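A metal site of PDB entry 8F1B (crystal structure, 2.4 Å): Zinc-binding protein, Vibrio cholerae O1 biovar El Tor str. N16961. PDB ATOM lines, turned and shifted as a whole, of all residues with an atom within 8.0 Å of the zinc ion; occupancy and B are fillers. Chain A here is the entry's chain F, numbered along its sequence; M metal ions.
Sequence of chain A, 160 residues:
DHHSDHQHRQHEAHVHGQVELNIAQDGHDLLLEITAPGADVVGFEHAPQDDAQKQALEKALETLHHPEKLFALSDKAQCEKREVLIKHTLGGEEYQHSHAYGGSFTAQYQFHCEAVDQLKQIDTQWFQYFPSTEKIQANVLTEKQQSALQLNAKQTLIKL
A ring nitrogen (NE2) of His 112 is in hydrogen-bond range of the side-chain carboxylate (OE1) of Glu 114 (2.7 Å). O of His 112 sits at hydrogen-bond distance from N of Glu 80 (3.0 Å). The backbone carbonyl oxygen of His 28 sits at hydrogen-bond distance from the backbone NH of Cys 113 (2.6 Å).
Three residues have an atom within 4 Å of the zinc ion: His 28, Asp 29 and His 112. The nearest printed residue that does not touch the zinc ion is Cys 113 (5.0 Å).
The zinc ion is bound by a ring nitrogen (ND1) of His 112 (1.9 Å), a ring nitrogen (ND1) of His 28 (2.0 Å) and the side-chain carboxylate of Asp 29 (2.0 Å). The zinc ion has three donor atoms within binding distance.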
ATOM      1  N   ASP A  26      31.081  14.097   8.642  1.00  0.00           N
ATOM      2  CA  ASP A  26      30.442  14.448   7.356  1.00  0.00           C
ATOM      3  C   ASP A  26      29.348  15.479   7.633  1.00  0.00           C
ATOM      4  O   ASP A  26      28.486  15.197   8.465  1.00  0.00           O
ATOM      5  CB  ASP A  26      29.898  13.215   6.644  1.00  0.00           C
ATOM      6  CG  ASP A  26      29.890  13.374   5.143  1.00  0.00           C
ATOM      7  OD1 ASP A  26      30.788  14.085   4.608  1.00  0.00           O
ATOM      8  OD2 ASP A  26      28.998  12.792   4.519  1.00  0.00           O
ATOM      9  N   GLY A  27      29.418  16.633   6.972  1.00  0.00           N
ATOM     10  CA  GLY A  27      28.559  17.805   7.237  1.00  0.00           C
ATOM     11  C   GLY A  27      28.684  18.261   8.674  1.00  0.00           C
ATOM     12  O   GLY A  27      29.808  18.503   9.133  1.00  0.00           O
ATOM     13  N   HIS A  28      27.558  18.311   9.388  1.00  0.00           N
ATOM     14  CA  HIS A  28      27.461  18.915  10.747  1.00  0.00           C
ATOM     15  C   HIS A  28      27.742  17.858  11.815  1.00  0.00           C
ATOM     16  O   HIS A  28      27.762  18.211  13.006  1.00  0.00           O
ATOM     17  CB  HIS A  28      26.078  19.545  10.973  1.00  0.00           C
ATOM     18  CG  HIS A  28      24.942  18.854  10.282  1.00  0.00           C
ATOM     19  ND1 HIS A  28      24.032  18.004  10.921  1.00  0.00           N
ATOM     20  CD2 HIS A  28      24.562  18.904   8.980  1.00  0.00           C
ATOM     21  CE1 HIS A  28      23.166  17.561  10.042  1.00  0.00           C
ATOM     22  NE2 HIS A  28      23.461  18.096   8.845  1.00  0.00           N
ATOM     23  N   ASP A  29      27.942  16.601  11.413  1.00  0.00           N
ATOM     24  CA  ASP A  29      27.914  15.474  12.382  1.00  0.00           C
ATOM     25  C   ASP A  29      29.294  14.843  12.484  1.00  0.00           C
ATOM     26  O   ASP A  29      29.949  14.651  11.430  1.00  0.00           O
ATOM     27  CB  ASP A  29      26.852  14.455  11.992  1.00  0.00           C
ATOM     28  CG  ASP A  29      25.486  15.088  11.847  1.00  0.00           C
ATOM     29  OD1 ASP A  29      25.083  15.762  12.795  1.00  0.00           O
ATOM     30  OD2 ASP A  29      24.875  14.938  10.780  1.00  0.00           O
ATOM     31  N   LEU A  30      29.710  14.526  13.709  1.00  0.00           N
ATOM     32  CA  LEU A  30      30.909  13.689  13.943  1.00  0.00           C
ATOM     33  C   LEU A  30      30.485  12.383  14.604  1.00  0.00           C
ATOM     34  O   LEU A  30      29.964  12.457  15.729  1.00  0.00           O
ATOM     35  CB  LEU A  30      31.910  14.432  14.821  1.00  0.00           C
ATOM     36  CG  LEU A  30      33.198  13.658  15.022  1.00  0.00           C
ATOM     37  CD1 LEU A  30      33.990  13.588  13.706  1.00  0.00           C
ATOM     38  CD2 LEU A  30      34.026  14.278  16.128  1.00  0.00           C
ATOM     39  N   GLU A  80      27.641  18.552  20.432  1.00  0.00           N
ATOM     40  CA  GLU A  80      26.942  18.028  21.641  1.00  0.00           C
ATOM     41  C   GLU A  80      26.237  16.724  21.278  1.00  0.00           C
ATOM     42  O   GLU A  80      25.734  16.588  20.147  1.00  0.00           O
ATOM     43  CB  GLU A  80      25.992  19.080  22.215  1.00  0.00           C
ATOM     44  CG  GLU A  80      26.715  20.364  22.588  1.00  0.00           C
ATOM     45  CD  GLU A  80      26.257  21.109  23.840  1.00  0.00           C
ATOM     46  OE1 GLU A  80      26.768  22.216  24.069  1.00  0.00           O
ATOM     47  OE2 GLU A  80      25.412  20.570  24.588  1.00  0.00           O
ATOM     48  N   ARG A  82      24.174  13.445  20.484  1.00  0.00           N
ATOM     49  CA  ARG A  82      22.870  13.302  19.796  1.00  0.00           C
ATOM     50  C   ARG A  82      22.419  11.845  19.789  1.00  0.00           C
ATOM     51  O   ARG A  82      21.206  11.624  19.839  1.00  0.00           O
ATOM     52  CB  ARG A  82      22.936  13.847  18.372  1.00  0.00           C
ATOM     53  CG  ARG A  82      23.064  15.367  18.331  1.00  0.00           C
ATOM     54  CD  ARG A  82      22.002  16.146  19.103  1.00  0.00           C
ATOM     55  NE  ARG A  82      22.345  17.569  19.151  1.00  0.00           N
ATOM     56  CZ  ARG A  82      21.665  18.562  18.588  1.00  0.00           C
ATOM     57  NH1 ARG A  82      20.542  18.322  17.931  1.00  0.00           N
ATOM     58  NH2 ARG A  82      22.099  19.812  18.694  1.00  0.00           N
ATOM     59  N   GLN A 110      27.418   9.816  18.362  1.00  0.00           N
ATOM     60  CA  GLN A 110      27.119  10.745  17.273  1.00  0.00           C
ATOM     61  C   GLN A 110      26.939  12.132  17.881  1.00  0.00           C
ATOM     62  O   GLN A 110      26.062  12.309  18.730  1.00  0.00           O
ATOM     63  CB  GLN A 110      25.875  10.277  16.532  1.00  0.00           C
ATOM     64  CG  GLN A 110      25.307  11.367  15.639  1.00  0.00           C
ATOM     65  CD  GLN A 110      24.708  10.765  14.387  1.00  0.00           C
ATOM     66  OE1 GLN A 110      25.026   9.636  14.014  1.00  0.00           O
ATOM     67  NE2 GLN A 110      23.869  11.538  13.724  1.00  0.00           N
ATOM     68  N   PHE A 111      27.764  13.079  17.468  1.00  0.00           N
ATOM     69  CA  PHE A 111      27.617  14.494  17.869  1.00  0.00           C
ATOM     70  C   PHE A 111      27.053  15.274  16.685  1.00  0.00           C
ATOM     71  O   PHE A 111      27.301  14.912  15.526  1.00  0.00           O
ATOM     72  CB  PHE A 111      28.958  15.062  18.332  1.00  0.00           C
ATOM     73  CG  PHE A 111      29.506  14.423  19.585  1.00  0.00           C
ATOM     74  CD1 PHE A 111      30.128  13.190  19.517  1.00  0.00           C
ATOM     75  CD2 PHE A 111      29.437  15.073  20.805  1.00  0.00           C
ATOM     76  CE1 PHE A 111      30.662  12.604  20.659  1.00  0.00           C
ATOM     77  CE2 PHE A 111      29.982  14.496  21.944  1.00  0.00           C
ATOM     78  CZ  PHE A 111      30.594  13.259  21.866  1.00  0.00           C
ATOM     79  N   HIS A 112      26.300  16.322  17.000  1.00  0.00           N
ATOM     80  CA  HIS A 112      25.992  17.402  16.029  1.00  0.00           C
ATOM     81  C   HIS A 112      26.870  18.595  16.387  1.00  0.00           C
ATOM     82  O   HIS A 112      26.841  19.035  17.537  1.00  0.00           O
ATOM     83  CB  HIS A 112      24.509  17.757  16.019  1.00  0.00           C
ATOM     84  CG  HIS A 112      24.207  18.941  15.168  1.00  0.00           C
ATOM     85  ND1 HIS A 112      23.586  18.843  13.936  1.00  0.00           N
ATOM     86  CD2 HIS A 112      24.477  20.258  15.355  1.00  0.00           C
ATOM     87  CE1 HIS A 112      23.455  20.048  13.414  1.00  0.00           C
ATOM     88  NE2 HIS A 112      23.996  20.922  14.259  1.00  0.00           N
ATOM     89  N   CYS A 113      27.668  19.051  15.432  1.00  0.00           N
ATOM     90  CA  CYS A 113      28.629  20.163  15.600  1.00  0.00           C
ATOM     91  C   CYS A 113      28.051  21.406  14.934  1.00  0.00           C
ATOM     92  O   CYS A 113      27.734  21.346  13.727  1.00  0.00           O
ATOM     93  CB  CYS A 113      29.980  19.809  15.011  1.00  0.00           C
ATOM     94  SG  CYS A 113      30.733  18.341  15.764  1.00  0.00           S
ATOM     95  N   GLU A 114      27.902  22.495  15.696  1.00  0.00           N
ATOM     96  CA  GLU A 114      27.440  23.799  15.132  1.00  0.00           C
ATOM     97  C   GLU A 114      28.580  24.431  14.330  1.00  0.00           C
ATOM     98  O   GLU A 114      28.292  25.150  13.365  1.00  0.00           O
ATOM     99  CB  GLU A 114      26.960  24.729  16.247  1.00  0.00           C
ATOM    100  CG  GLU A 114      25.796  24.162  17.041  1.00  0.00           C
ATOM    101  CD  GLU A 114      24.539  23.951  16.232  1.00  0.00           C
ATOM    102  OE1 GLU A 114      24.617  23.394  15.103  1.00  0.00           O
ATOM    103  OE2 GLU A 114      23.471  24.317  16.725  1.00  0.00           O
HETATM  104 ZN    ZN M   1      23.771  17.310  12.757  1.00  0.00          ZN
